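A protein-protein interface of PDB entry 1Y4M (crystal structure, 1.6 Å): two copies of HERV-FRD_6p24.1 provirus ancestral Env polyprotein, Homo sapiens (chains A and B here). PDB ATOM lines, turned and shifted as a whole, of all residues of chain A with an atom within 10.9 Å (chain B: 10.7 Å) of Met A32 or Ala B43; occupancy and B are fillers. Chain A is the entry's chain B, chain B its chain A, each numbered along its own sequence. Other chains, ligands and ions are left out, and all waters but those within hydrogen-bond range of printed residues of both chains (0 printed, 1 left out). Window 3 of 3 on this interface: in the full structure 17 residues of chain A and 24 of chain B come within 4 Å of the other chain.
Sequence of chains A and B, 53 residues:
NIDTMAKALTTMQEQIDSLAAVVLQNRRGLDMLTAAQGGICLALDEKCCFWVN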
ATOM      1  N   VAL A  23      -2.420 -23.334 -29.683  1.00  0.00           N
ATOM      2  CA  VAL A  23      -1.037 -23.252 -29.244  1.00  0.00           C
ATOM      3  C   VAL A  23      -0.255 -22.195 -29.990  1.00  0.00           C
ATOM      4  O   VAL A  23       0.475 -21.415 -29.386  1.00  0.00           O
ATOM      5  CB  VAL A  23      -0.323 -24.585 -29.430  1.00  0.00           C
ATOM      6  CG1 VAL A  23       1.134 -24.458 -29.013  1.00  0.00           C
ATOM      7  CG2 VAL A  23      -1.021 -25.645 -28.611  1.00  0.00           C
ATOM      8  N   LEU A  24      -0.397 -22.186 -31.307  1.00  0.00           N
ATOM      9  CA  LEU A  24       0.315 -21.213 -32.114  1.00  0.00           C
ATOM     10  C   LEU A  24      -0.163 -19.817 -31.757  1.00  0.00           C
ATOM     11  O   LEU A  24       0.618 -18.868 -31.737  1.00  0.00           O
ATOM     12  CB  LEU A  24       0.084 -21.482 -33.597  1.00  0.00           C
ATOM     13  CG  LEU A  24       0.574 -22.842 -34.101  1.00  0.00           C
ATOM     14  CD1 LEU A  24       0.234 -22.980 -35.583  1.00  0.00           C
ATOM     15  CD2 LEU A  24       2.074 -22.974 -33.876  1.00  0.00           C
ATOM     16  N   GLN A  25      -1.447 -19.691 -31.469  1.00  0.00           N
ATOM     17  CA  GLN A  25      -1.982 -18.390 -31.112  1.00  0.00           C
ATOM     18  C   GLN A  25      -1.422 -17.993 -29.757  1.00  0.00           C
ATOM     19  O   GLN A  25      -1.091 -16.838 -29.519  1.00  0.00           O
ATOM     20  CB  GLN A  25      -3.499 -18.445 -31.076  1.00  0.00           C
ATOM     21  CG  GLN A  25      -4.121 -17.133 -30.710  1.00  0.00           C
ATOM     22  CD  GLN A  25      -5.583 -17.116 -31.029  1.00  0.00           C
ATOM     23  OE1 GLN A  25      -6.352 -17.908 -30.488  1.00  0.00           O
ATOM     24  NE2 GLN A  25      -5.982 -16.226 -31.927  1.00  0.00           N
ATOM     25  N   ASN A  26      -1.325 -18.964 -28.860  1.00  0.00           N
ATOM     26  CA  ASN A  26      -0.775 -18.683 -27.554  1.00  0.00           C
ATOM     27  C   ASN A  26       0.660 -18.251 -27.729  1.00  0.00           C
ATOM     28  O   ASN A  26       1.133 -17.369 -27.029  1.00  0.00           O
ATOM     29  CB  ASN A  26      -0.813 -19.922 -26.682  1.00  0.00           C
ATOM     30  CG  ASN A  26      -2.183 -20.190 -26.131  1.00  0.00           C
ATOM     31  OD1 ASN A  26      -3.104 -19.397 -26.323  1.00  0.00           O
ATOM     32  ND2 ASN A  26      -2.331 -21.304 -25.426  1.00  0.00           N
ATOM     33  N   ARG A  27       1.348 -18.884 -28.670  1.00  0.00           N
ATOM     34  CA  ARG A  27       2.726 -18.523 -28.924  1.00  0.00           C
ATOM     35  C   ARG A  27       2.806 -17.093 -29.446  1.00  0.00           C
ATOM     36  O   ARG A  27       3.672 -16.343 -29.023  1.00  0.00           O
ATOM     37  CB  ARG A  27       3.374 -19.490 -29.913  1.00  0.00           C
ATOM     38  CG  ARG A  27       4.734 -19.013 -30.409  1.00  0.00           C
ATOM     39  CD  ARG A  27       5.677 -18.706 -29.261  1.00  0.00           C
ATOM     40  NE  ARG A  27       5.868 -19.875 -28.407  1.00  0.00           N
ATOM     41  CZ  ARG A  27       6.825 -20.775 -28.585  1.00  0.00           C
ATOM     42  NH1 ARG A  27       7.688 -20.637 -29.582  1.00  0.00           N
ATOM     43  NH2 ARG A  27       6.910 -21.818 -27.780  1.00  0.00           N
ATOM     44  N   ARG A  28       1.901 -16.708 -30.345  1.00  0.00           N
ATOM     45  CA  ARG A  28       1.925 -15.341 -30.852  1.00  0.00           C
ATOM     46  C   ARG A  28       1.607 -14.378 -29.722  1.00  0.00           C
ATOM     47  O   ARG A  28       2.147 -13.273 -29.657  1.00  0.00           O
ATOM     48  CB  ARG A  28       0.915 -15.164 -31.983  1.00  0.00           C
ATOM     49  CG  ARG A  28       1.258 -15.958 -33.225  1.00  0.00           C
ATOM     50  CD  ARG A  28       0.389 -15.521 -34.394  1.00  0.00           C
ATOM     51  NE  ARG A  28      -1.007 -15.861 -34.197  1.00  0.00           N
ATOM     52  CZ  ARG A  28      -1.518 -17.070 -34.396  1.00  0.00           C
ATOM     53  NH1 ARG A  28      -0.740 -18.065 -34.804  1.00  0.00           N
ATOM     54  NH2 ARG A  28      -2.810 -17.285 -34.191  1.00  0.00           N
ATOM     55  N   GLY A  29       0.732 -14.812 -28.825  1.00  0.00           N
ATOM     56  CA  GLY A  29       0.366 -13.988 -27.694  1.00  0.00           C
ATOM     57  C   GLY A  29       1.584 -13.782 -26.820  1.00  0.00           C
ATOM     58  O   GLY A  29       1.879 -12.674 -26.386  1.00  0.00           O
ATOM     59  N   LEU A  30       2.308 -14.865 -26.567  1.00  0.00           N
ATOM     60  CA  LEU A  30       3.488 -14.758 -25.736  1.00  0.00           C
ATOM     61  C   LEU A  30       4.577 -13.940 -26.405  1.00  0.00           C
ATOM     62  O   LEU A  30       5.297 -13.209 -25.739  1.00  0.00           O
ATOM     63  CB  LEU A  30       4.024 -16.142 -25.400  1.00  0.00           C
ATOM     64  CG  LEU A  30       3.200 -16.874 -24.355  1.00  0.00           C
ATOM     65  CD1 LEU A  30       3.579 -18.349 -24.373  1.00  0.00           C
ATOM     66  CD2 LEU A  30       3.413 -16.255 -22.978  1.00  0.00           C
ATOM     67  N   ASP A  31       4.709 -14.070 -27.721  1.00  0.00           N
ATOM     68  CA  ASP A  31       5.727 -13.314 -28.423  1.00  0.00           C
ATOM     69  C   ASP A  31       5.387 -11.840 -28.374  1.00  0.00           C
ATOM     70  O   ASP A  31       6.266 -10.990 -28.326  1.00  0.00           O
ATOM     71  CB  ASP A  31       5.851 -13.777 -29.867  1.00  0.00           C
ATOM     72  CG  ASP A  31       6.681 -15.027 -29.988  1.00  0.00           C
ATOM     73  OD1 ASP A  31       7.535 -15.225 -29.102  1.00  0.00           O
ATOM     74  OD2 ASP A  31       6.499 -15.797 -30.957  1.00  0.00           O
ATOM     75  N   MET A  32       4.098 -11.540 -28.388  1.00  0.00           N
ATOM     76  CA  MET A  32       3.680 -10.154 -28.323  1.00  0.00           C
ATOM     77  C   MET A  32       3.991  -9.607 -26.938  1.00  0.00           C
ATOM     78  O   MET A  32       4.560  -8.530 -26.798  1.00  0.00           O
ATOM     79  CB  MET A  32       2.190 -10.050 -28.598  1.00  0.00           C
ATOM     80  CG  MET A  32       1.637  -8.665 -28.376  1.00  0.00           C
ATOM     81  SD  MET A  32      -0.135  -8.719 -28.604  1.00  0.00           S
ATOM     82  CE  MET A  32      -0.632  -9.305 -27.011  1.00  0.00           C
ATOM     83  N   LEU A  33       3.622 -10.362 -25.908  1.00  0.00           N
ATOM     84  CA  LEU A  33       3.863  -9.921 -24.539  1.00  0.00           C
ATOM     85  C   LEU A  33       5.333  -9.761 -24.205  1.00  0.00           C
ATOM     86  O   LEU A  33       5.680  -9.071 -23.252  1.00  0.00           O
ATOM     87  CB  LEU A  33       3.246 -10.902 -23.555  1.00  0.00           C
ATOM     88  CG  LEU A  33       1.729 -11.012 -23.621  1.00  0.00           C
ATOM     89  CD1 LEU A  33       1.300 -12.113 -22.692  1.00  0.00           C
ATOM     90  CD2 LEU A  33       1.073  -9.683 -23.246  1.00  0.00           C
ATOM     91  N   THR A  34       6.197 -10.415 -24.970  1.00  0.00           N
ATOM     92  CA  THR A  34       7.624 -10.320 -24.709  1.00  0.00           C
ATOM     93  C   THR A  34       8.365  -9.803 -25.926  1.00  0.00           C
ATOM     94  O   THR A  34       9.552 -10.070 -26.099  1.00  0.00           O
ATOM     95  CB  THR A  34       8.206 -11.688 -24.320  1.00  0.00           C
ATOM     96  OG1 THR A  34       7.956 -12.627 -25.370  1.00  0.00           O
ATOM     97  CG2 THR A  34       7.560 -12.193 -23.037  1.00  0.00           C
ATOM     98  N   ALA A  35       7.668  -9.057 -26.772  1.00  0.00           N
ATOM     99  CA  ALA A  35       8.283  -8.530 -27.978  1.00  0.00           C
ATOM    100  C   ALA A  35       9.544  -7.732 -27.667  1.00  0.00           C
ATOM    101  O   ALA A  35      10.537  -7.837 -28.378  1.00  0.00           O
ATOM    102  CB  ALA A  35       7.280  -7.667 -28.730  1.00  0.00           C
ATOM    103  N   ALA A  36       9.496  -6.949 -26.593  1.00  0.00           N
ATOM    104  CA  ALA A  36      10.629  -6.127 -26.182  1.00  0.00           C
ATOM    105  C   ALA A  36      11.820  -6.986 -25.789  1.00  0.00           C
ATOM    106  O   ALA A  36      12.962  -6.538 -25.842  1.00  0.00           O
ATOM    107  CB  ALA A  36      10.229  -5.234 -25.009  1.00  0.00           C
ATOM    108  N   GLN A  37      11.542  -8.222 -25.386  1.00  0.00           N
ATOM    109  CA  GLN A  37      12.590  -9.143 -24.976  1.00  0.00           C
ATOM    110  C   GLN A  37      13.003 -10.053 -26.120  1.00  0.00           C
ATOM    111  O   GLN A  37      13.796 -10.974 -25.927  1.00  0.00           O
ATOM    112  CB  GLN A  37      12.119 -10.004 -23.805  1.00  0.00           C
ATOM    113  CG  GLN A  37      11.976  -9.273 -22.478  1.00  0.00           C
ATOM    114  CD  GLN A  37      10.798  -8.330 -22.447  1.00  0.00           C
ATOM    115  OE1 GLN A  37       9.726  -8.644 -22.961  1.00  0.00           O
ATOM    116  NE2 GLN A  37      10.986  -7.167 -21.830  1.00  0.00           N
ATOM    117  N   GLY A  38      12.451  -9.803 -27.302  1.00  0.00           N
ATOM    118  CA  GLY A  38      12.791 -10.606 -28.461  1.00  0.00           C
ATOM    119  C   GLY A  38      11.892 -11.803 -28.698  1.00  0.00           C
ATOM    120  O   GLY A  38      12.212 -12.673 -29.508  1.00  0.00           O
ATOM    121  N   GLY A  39      10.758 -11.854 -28.019  1.00  0.00           N
ATOM    122  CA  GLY A  39       9.888 -12.993 -28.220  1.00  0.00           C
ATOM    123  C   GLY A  39      10.013 -13.874 -27.004  1.00  0.00           C
ATOM    124  O   GLY A  39      10.955 -13.744 -26.222  1.00  0.00           O
ATOM    125  N   ILE A  40       9.094 -14.817 -26.873  1.00  0.00           N
ATOM    126  CA  ILE A  40       9.100 -15.653 -25.692  1.00  0.00           C
ATOM    127  C   ILE A  40      10.295 -16.575 -25.622  1.00  0.00           C
ATOM    128  O   ILE A  40      10.812 -16.854 -24.539  1.00  0.00           O
ATOM    129  CB  ILE A  40       7.775 -16.437 -25.565  1.00  0.00           C
ATOM    130  CG1 ILE A  40       7.585 -16.861 -24.109  1.00  0.00           C
ATOM    131  CG2 ILE A  40       7.724 -17.602 -26.551  1.00  0.00           C
ATOM    132  CD1 ILE A  40       7.365 -15.677 -23.195  1.00  0.00           C
ATOM    133  N   CYS A  41      10.749 -17.037 -26.772  1.00  0.00           N
ATOM    134  CA  CYS A  41      11.896 -17.919 -26.792  1.00  0.00           C
ATOM    135  C   CYS A  41      13.156 -17.214 -26.350  1.00  0.00           C
ATOM    136  O   CYS A  41      13.913 -17.738 -25.547  1.00  0.00           O
ATOM    137  CB  CYS A  41      12.058 -18.501 -28.175  1.00  0.00           C
ATOM    138  SG  CYS A  41      10.833 -19.796 -28.454  1.00  0.00           S
ATOM    139  N   LEU A  42      13.378 -16.014 -26.874  1.00  0.00           N
ATOM    140  CA  LEU A  42      14.550 -15.258 -26.475  1.00  0.00           C
ATOM    141  C   LEU A  42      14.408 -14.836 -25.024  1.00  0.00           C
ATOM    142  O   LEU A  42      15.380 -14.810 -24.277  1.00  0.00           O
ATOM    143  CB  LEU A  42      14.724 -14.019 -27.342  1.00  0.00           C
ATOM    144  CG  LEU A  42      15.401 -14.297 -28.674  1.00  0.00           C
ATOM    145  CD1 LEU A  42      15.470 -13.005 -29.461  1.00  0.00           C
ATOM    146  CD2 LEU A  42      16.806 -14.861 -28.444  1.00  0.00           C
ATOM    147  N   ALA A  43      13.187 -14.501 -24.624  1.00  0.00           N
ATOM    148  CA  ALA A  43      12.955 -14.091 -23.252  1.00  0.00           C
ATOM    149  C   ALA A  43      13.246 -15.285 -22.357  1.00  0.00           C
ATOM    150  O   ALA A  43      13.805 -15.140 -21.275  1.00  0.00           O
ATOM    151  CB  ALA A  43      11.524 -13.647 -23.071  1.00  0.00           C
ATOM    152  N   ARG B  27      -3.851 -20.745 -22.210  1.00  0.00           N
ATOM    153  CA  ARG B  27      -4.701 -19.745 -22.822  1.00  0.00           C
ATOM    154  C   ARG B  27      -5.335 -18.898 -21.736  1.00  0.00           C
ATOM    155  O   ARG B  27      -5.432 -17.691 -21.875  1.00  0.00           O
ATOM    156  CB  ARG B  27      -5.785 -20.408 -23.668  1.00  0.00           C
ATOM    157  CG  ARG B  27      -6.844 -19.433 -24.148  1.00  0.00           C
ATOM    158  CD  ARG B  27      -6.223 -18.258 -24.886  1.00  0.00           C
ATOM    159  NE  ARG B  27      -5.529 -18.667 -26.100  1.00  0.00           N
ATOM    160  CZ  ARG B  27      -6.116 -18.843 -27.279  1.00  0.00           C
ATOM    161  NH1 ARG B  27      -7.422 -18.635 -27.413  1.00  0.00           N
ATOM    162  NH2 ARG B  27      -5.402 -19.239 -28.324  1.00  0.00           N
ATOM    163  N   GLY B  29      -4.097 -18.347 -18.929  1.00  0.00           N
ATOM    164  CA  GLY B  29      -3.015 -17.526 -18.429  1.00  0.00           C
ATOM    165  C   GLY B  29      -2.828 -16.302 -19.304  1.00  0.00           C
ATOM    166  O   GLY B  29      -2.681 -15.190 -18.807  1.00  0.00           O
ATOM    167  N   LEU B  30      -2.834 -16.507 -20.615  1.00  0.00           N
ATOM    168  CA  LEU B  30      -2.670 -15.402 -21.547  1.00  0.00           C
ATOM    169  C   LEU B  30      -3.840 -14.444 -21.507  1.00  0.00           C
ATOM    170  O   LEU B  30      -3.661 -13.233 -21.629  1.00  0.00           O
ATOM    171  CB  LEU B  30      -2.500 -15.932 -22.961  1.00  0.00           C
ATOM    172  CG  LEU B  30      -1.095 -16.468 -23.232  1.00  0.00           C
ATOM    173  CD1 LEU B  30      -1.089 -17.234 -24.543  1.00  0.00           C
ATOM    174  CD2 LEU B  30      -0.097 -15.317 -23.269  1.00  0.00           C
ATOM    175  N   ASP B  31      -5.042 -14.982 -21.353  1.00  0.00           N
ATOM    176  CA  ASP B  31      -6.218 -14.130 -21.289  1.00  0.00           C
ATOM    177  C   ASP B  31      -6.153 -13.291 -20.029  1.00  0.00           C
ATOM    178  O   ASP B  31      -6.550 -12.126 -20.023  1.00  0.00           O
ATOM    179  CB  ASP B  31      -7.493 -14.970 -21.296  1.00  0.00           C
ATOM    180  CG  ASP B  31      -7.808 -15.525 -22.665  1.00  0.00           C
ATOM    181  OD1 ASP B  31      -7.435 -14.857 -23.651  1.00  0.00           O
ATOM    182  OD2 ASP B  31      -8.430 -16.606 -22.756  1.00  0.00           O
ATOM    183  N   MET B  32      -5.643 -13.890 -18.963  1.00  0.00           N
ATOM    184  CA  MET B  32      -5.522 -13.186 -17.706  1.00  0.00           C
ATOM    185  C   MET B  32      -4.508 -12.053 -17.840  1.00  0.00           C
ATOM    186  O   MET B  32      -4.747 -10.944 -17.379  1.00  0.00           O
ATOM    187  CB  MET B  32      -5.109 -14.166 -16.609  1.00  0.00           C
ATOM    188  CG  MET B  32      -4.978 -13.552 -15.238  1.00  0.00           C
ATOM    189  SD  MET B  32      -3.358 -12.828 -15.004  1.00  0.00           S
ATOM    190  CE  MET B  32      -2.381 -14.308 -14.719  1.00  0.00           C
ATOM    191  N   LEU B  33      -3.384 -12.333 -18.492  1.00  0.00           N
ATOM    192  CA  LEU B  33      -2.347 -11.325 -18.672  1.00  0.00           C
ATOM    193  C   LEU B  33      -2.780 -10.188 -19.577  1.00  0.00           C
ATOM    194  O   LEU B  33      -2.234  -9.091 -19.508  1.00  0.00           O
ATOM    195  CB  LEU B  33      -1.087 -11.959 -19.245  1.00  0.00           C
ATOM    196  CG  LEU B  33      -0.335 -12.838 -18.245  1.00  0.00           C
ATOM    197  CD1 LEU B  33       0.661 -13.694 -19.002  1.00  0.00           C
ATOM    198  CD2 LEU B  33       0.358 -11.973 -17.210  1.00  0.00           C
ATOM    199  N   THR B  34      -3.768 -10.448 -20.421  1.00  0.00           N
ATOM    200  CA  THR B  34      -4.246  -9.429 -21.342  1.00  0.00           C
ATOM    201  C   THR B  34      -5.704  -9.107 -21.076  1.00  0.00           C
ATOM    202  O   THR B  34      -6.422  -8.656 -21.965  1.00  0.00           O
ATOM    203  CB  THR B  34      -4.088  -9.904 -22.783  1.00  0.00           C
ATOM    204  OG1 THR B  34      -4.754 -11.163 -22.943  1.00  0.00           O
ATOM    205  CG2 THR B  34      -2.608 -10.071 -23.117  1.00  0.00           C
ATOM    206  N   ALA B  35      -6.132  -9.341 -19.841  1.00  0.00           N
ATOM    207  CA  ALA B  35      -7.510  -9.091 -19.446  1.00  0.00           C
ATOM    208  C   ALA B  35      -7.968  -7.679 -19.792  1.00  0.00           C
ATOM    209  O   ALA B  35      -9.097  -7.483 -20.248  1.00  0.00           O
ATOM    210  CB  ALA B  35      -7.671  -9.340 -17.956  1.00  0.00           C
ATOM    211  N   ALA B  36      -7.096  -6.700 -19.575  1.00  0.00           N
ATOM    212  CA  ALA B  36      -7.434  -5.308 -19.862  1.00  0.00           C
ATOM    213  C   ALA B  36      -7.704  -5.108 -21.343  1.00  0.00           C
ATOM    214  O   ALA B  36      -8.464  -4.223 -21.730  1.00  0.00           O
ATOM    215  CB  ALA B  36      -6.310  -4.390 -19.414  1.00  0.00           C
ATOM    216  N   GLN B  37      -7.076  -5.935 -22.167  1.00  0.00           N
ATOM    217  CA  GLN B  37      -7.240  -5.842 -23.608  1.00  0.00           C
ATOM    218  C   GLN B  37      -8.338  -6.763 -24.114  1.00  0.00           C
ATOM    219  O   GLN B  37      -8.556  -6.874 -25.320  1.00  0.00           O
ATOM    220  CB  GLN B  37      -5.927  -6.187 -24.309  1.00  0.00           C
ATOM    221  CG  GLN B  37      -4.792  -5.218 -24.028  1.00  0.00           C
ATOM    222  CD  GLN B  37      -3.578  -5.493 -24.888  1.00  0.00           C
ATOM    223  OE1 GLN B  37      -3.629  -5.362 -26.113  1.00  0.00           O
ATOM    224  NE2 GLN B  37      -2.480  -5.883 -24.256  1.00  0.00           N
ATOM    225  N   GLY B  38      -9.018  -7.434 -23.191  1.00  0.00           N
ATOM    226  CA  GLY B  38     -10.085  -8.331 -23.580  1.00  0.00           C
ATOM    227  C   GLY B  38      -9.631  -9.736 -23.925  1.00  0.00           C
ATOM    228  O   GLY B  38     -10.314 -10.447 -24.656  1.00  0.00           O
ATOM    229  N   GLY B  39      -8.489 -10.155 -23.397  1.00  0.00           N
ATOM    230  CA  GLY B  39      -8.028 -11.493 -23.708  1.00  0.00           C
ATOM    231  C   GLY B  39      -6.933 -11.458 -24.745  1.00  0.00           C
ATOM    232  O   GLY B  39      -6.770 -10.470 -25.459  1.00  0.00           O
ATOM    233  N   ILE B  40      -6.197 -12.558 -24.852  1.00  0.00           N
ATOM    234  CA  ILE B  40      -5.082 -12.630 -25.779  1.00  0.00           C
ATOM    235  C   ILE B  40      -5.483 -12.512 -27.242  1.00  0.00           C
ATOM    236  O   ILE B  40      -4.765 -11.908 -28.034  1.00  0.00           O
ATOM    237  CB  ILE B  40      -4.290 -13.936 -25.559  1.00  0.00           C
ATOM    238  CG1 ILE B  40      -2.898 -13.801 -26.165  1.00  0.00           C
ATOM    239  CG2 ILE B  40      -5.029 -15.110 -26.169  1.00  0.00           C
ATOM    240  CD1 ILE B  40      -2.068 -12.711 -25.520  1.00  0.00           C
ATOM    241  N   CYS B  41      -6.626 -13.090 -27.593  1.00  0.00           N
ATOM    242  CA  CYS B  41      -7.121 -13.041 -28.960  1.00  0.00           C
ATOM    243  C   CYS B  41      -7.394 -11.606 -29.364  1.00  0.00           C
ATOM    244  O   CYS B  41      -6.951 -11.150 -30.414  1.00  0.00           O
ATOM    245  CB  CYS B  41      -8.405 -13.853 -29.088  1.00  0.00           C
ATOM    246  SG  CYS B  41      -8.155 -15.650 -28.974  1.00  0.00           S
ATOM    247  N   LEU B  42      -8.131 -10.891 -28.530  1.00  0.00           N
ATOM    248  CA  LEU B  42      -8.427  -9.505 -28.843  1.00  0.00           C
ATOM    249  C   LEU B  42      -7.144  -8.689 -28.745  1.00  0.00           C
ATOM    250  O   LEU B  42      -6.948  -7.740 -29.497  1.00  0.00           O
ATOM    251  CB  LEU B  42      -9.508  -8.967 -27.906  1.00  0.00           C
ATOM    252  CG  LEU B  42     -10.878  -9.631 -28.126  1.00  0.00           C
ATOM    253  CD1 LEU B  42     -11.858  -9.160 -27.070  1.00  0.00           C
ATOM    254  CD2 LEU B  42     -11.395  -9.303 -29.525  1.00  0.00           C
ATOM    255  N   ALA B  43      -6.259  -9.065 -27.827  1.00  0.00           N
ATOM    256  CA  ALA B  43      -4.997  -8.349 -27.677  1.00  0.00           C
ATOM    257  C   ALA B  43      -4.158  -8.537 -28.932  1.00  0.00           C
ATOM    258  O   ALA B  43      -3.391  -7.659 -29.322  1.00  0.00           O
ATOM    259  CB  ALA B  43      -4.236  -8.870 -26.459  1.00  0.00           C
ATOM    260  N   LEU B  44      -4.301  -9.700 -29.559  1.00  0.00           N
ATOM    261  CA  LEU B  44      -3.560 -10.009 -30.773  1.00  0.00           C
ATOM    262  C   LEU B  44      -4.320  -9.564 -32.005  1.00  0.00           C
ATOM    263  O   LEU B  44      -3.829  -9.722 -33.115  1.00  0.00           O
ATOM    264  CB  LEU B  44      -3.316 -11.515 -30.877  1.00  0.00           C
ATOM    265  CG  LEU B  44      -2.287 -12.152 -29.946  1.00  0.00           C
ATOM    266  CD1 LEU B  44      -2.439 -13.651 -30.003  1.00  0.00           C
ATOM    267  CD2 LEU B  44      -0.890 -11.735 -30.355  1.00  0.00           C
ATOM    268  N   ASP B  45      -5.511  -9.009 -31.802  1.00  0.00           N
ATOM    269  CA  ASP B  45      -6.358  -8.578 -32.909  1.00  0.00           C
ATOM    270  C   ASP B  45      -6.530  -9.745 -33.879  1.00  0.00           C
ATOM    271  O   ASP B  45      -6.432  -9.590 -35.096  1.00  0.00           O
ATOM    272  CB  ASP B  45      -5.759  -7.346 -33.615  1.00  0.00           C
ATOM    273  CG  ASP B  45      -4.404  -7.617 -34.256  1.00  0.00           C
ATOM    274  OD1 ASP B  45      -4.354  -8.320 -35.289  1.00  0.00           O
ATOM    275  OD2 ASP B  45      -3.384  -7.119 -33.729  1.00  0.00           O
ATOM    276  N   GLU B  46      -6.802 -10.922 -33.321  1.00  0.00           N
ATOM    277  CA  GLU B  46      -6.993 -12.132 -34.115  1.00  0.00           C
ATOM    278  C   GLU B  46      -8.283 -12.853 -33.757  1.00  0.00           C
ATOM    279  O   GLU B  46      -8.865 -12.630 -32.697  1.00  0.00           O
ATOM    280  CB  GLU B  46      -5.845 -13.113 -33.881  1.00  0.00           C
ATOM    281  CG  GLU B  46      -4.470 -12.639 -34.271  1.00  0.00           C
ATOM    282  CD  GLU B  46      -3.406 -13.660 -33.906  1.00  0.00           C
ATOM    283  OE1 GLU B  46      -3.783 -14.761 -33.445  1.00  0.00           O
ATOM    284  OE2 GLU B  46      -2.208 -13.372 -34.080  1.00  0.00           O
ATOM    285  N   LYS B  47      -8.714 -13.730 -34.656  1.00  0.00           N
ATOM    286  CA  LYS B  47      -9.905 -14.527 -34.429  1.00  0.00           C
ATOM    287  C   LYS B  47      -9.455 -15.530 -33.374  1.00  0.00           C
ATOM    288  O   LYS B  47      -8.367 -16.097 -33.482  1.00  0.00           O
ATOM    289  CB  LYS B  47     -10.308 -15.265 -35.706  1.00  0.00           C
ATOM    290  CG  LYS B  47     -11.596 -16.070 -35.578  1.00  0.00           C
ATOM    291  CD  LYS B  47     -11.870 -16.915 -36.812  1.00  0.00           C
ATOM    292  CE  LYS B  47     -10.812 -17.995 -36.987  1.00  0.00           C
ATOM    293  NZ  LYS B  47     -11.091 -18.851 -38.175  1.00  0.00           N
ATOM    294  N   CYS B  48     -10.278 -15.749 -32.359  1.00  0.00           N
ATOM    295  CA  CYS B  48      -9.912 -16.674 -31.296  1.00  0.00           C
ATOM    296  C   CYS B  48      -9.926 -18.130 -31.728  1.00  0.00           C
ATOM    297  O   CYS B  48     -10.873 -18.589 -32.365  1.00  0.00           O
ATOM    298  CB  CYS B  48     -10.848 -16.495 -30.107  1.00  0.00           C
ATOM    299  SG  CYS B  48     -10.005 -16.348 -28.499  1.00  0.00           S
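Among the printed residues, pairs that only touch across the chains: Asn A26 with Leu B30, Arg A28 with Leu B44, Gln A25 with Leu B44, Gly A29 with Ile B40, Leu A33 with Leu B30, Met A32 with Leu B44, Gly A29 with Leu B44, Leu A30 with Leu B30, Leu A33 with Thr B34, Gln A25 with Cys B48 and Met A32 with Ile B40.
Printed residues of chain B that touch a printed residue of chain A: Arg B27, Leu B30, Thr B34, Ile B40, Cys B41, Ala B43, Leu B44, Glu B46, Lys B47 and Cys B48. Hydrophobic or aromatic side chains of chain B within 4 Å of the printed part of chain A: Leu B30, Ile B40, Ala B43 and Leu B44. Of the 21 printed residues of chain A, 7 touch a printed residue of chain B. Printed residues of chain A that touch a printed residue of chain B: Gln A25, Asn A26, Arg A28, Gly A29, Leu A30, Met A32 and Leu A33. Hydrophobic or aromatic side chains of chain A within 4 Å of the printed part of chain B: Leu A30, Met A32 and Leu A33. Among the printed residues, 18 pairs touch across the chains. Among the printed residues, Asp or Glu carboxylates within 4 Å of a Lys or Arg side-chain nitrogen of the other chain: Arg A28 with Glu B46 (2.8 Å).
The side-chain amide oxygen (OE1) of Gln A25 lies within hydrogen-bond range of the guanidinium group (NH2) of Arg B27. The side-chain amide oxygen (OD1) of Asn A26 sits at hydrogen-bond distance from the guanidinium group (NE) of Arg B27, at 2.5 Å. The side-chain sulfur (SG) of Cys B41 lies close to the side-chain amide oxygen (OE1) of Gln A25 (3.3 Å). The side-chain carboxylate of Glu B46 sits at hydrogen-bond distance from the side-chain amide nitrogen of Gln A25. The guanidinium group of Arg A28 lies within salt-bridge range of the side-chain carboxylate of Glu B46, at 2.8 Å. O of Lys B47 is in hydrogen-bond range of NE2 of Gln A25 (2.9 Å). O of Ala B43 lies close to SD of Met A32.
Gly A29 touches Ile B40, but with the chains exchanged Ile A40 does not touch Gly B29 (10.9 Å). Met A32 touches Ala B43, but with the chains exchanged Ala A43 does not touch Met B32 (16.2 Å). Leu A33 touches Leu B30, but with the chains exchanged Leu A30 does not touch Leu B33 (5.5 Å). Leu A33 touches Thr B34, but with the chains exchanged Thr A34 does not touch Leu B33 (8.1 Å). 16 positions are printed for both chains.
O of Leu B30 is in hydrogen-bond range of OG1 of Thr B34. N of Ile B40 is in hydrogen-bond range of OD1 of Asp B31 (2.9 Å). The backbone NH (N) of Ile B40 sits at hydrogen-bond distance from the side-chain hydroxyl (OG1) of Thr B34 (2.8 Å). The guanidinium group (NH1) of Arg A28 sits close to the backbone carbonyl oxygen (O) of Leu A24 (3.4 Å). O of Leu A30 is in hydrogen-bond range of OG1 of Thr A34, at 2.7 Å.
Of the printed residues of chain B, Met A32 touches Ile B40, Ala B43 and Leu B44. Ala B43 touches just one residue of chain A: Met A32 (3.5 Å). Of the printed residues of chain B, Gly A29 touches Ile B40 (3.5 Å) and Leu B44 (3.6 Å). No residue of chain B comes within 4 Å of Asp A31. No residue of chain B comes within 4 Å of Thr A34. No residue of chain B comes within 4 Å of Ala A35. Thr B34 touches just one residue of chain A: Leu A33. Gly B38 touches none of the printed residues of chain A. Gly B39 touches none of the printed residues of chain A. No residue of chain A comes within 4 Å of Asp B45. Of the printed residues of chain B, Gln A25 touches Arg B27 (2.7 Å), Cys B41 (3.3 Å), Leu B44 (3.5 Å), Glu B46 (3.0 Å), Lys B47 (2.9 Å) and Cys B48 (3.8 Å). Printed residues of chain A within 4 Å of Cys B48: Gln A25. The nearest printed residue of chain B that does not touch Met A32 is Thr B34 (4.4 Å).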
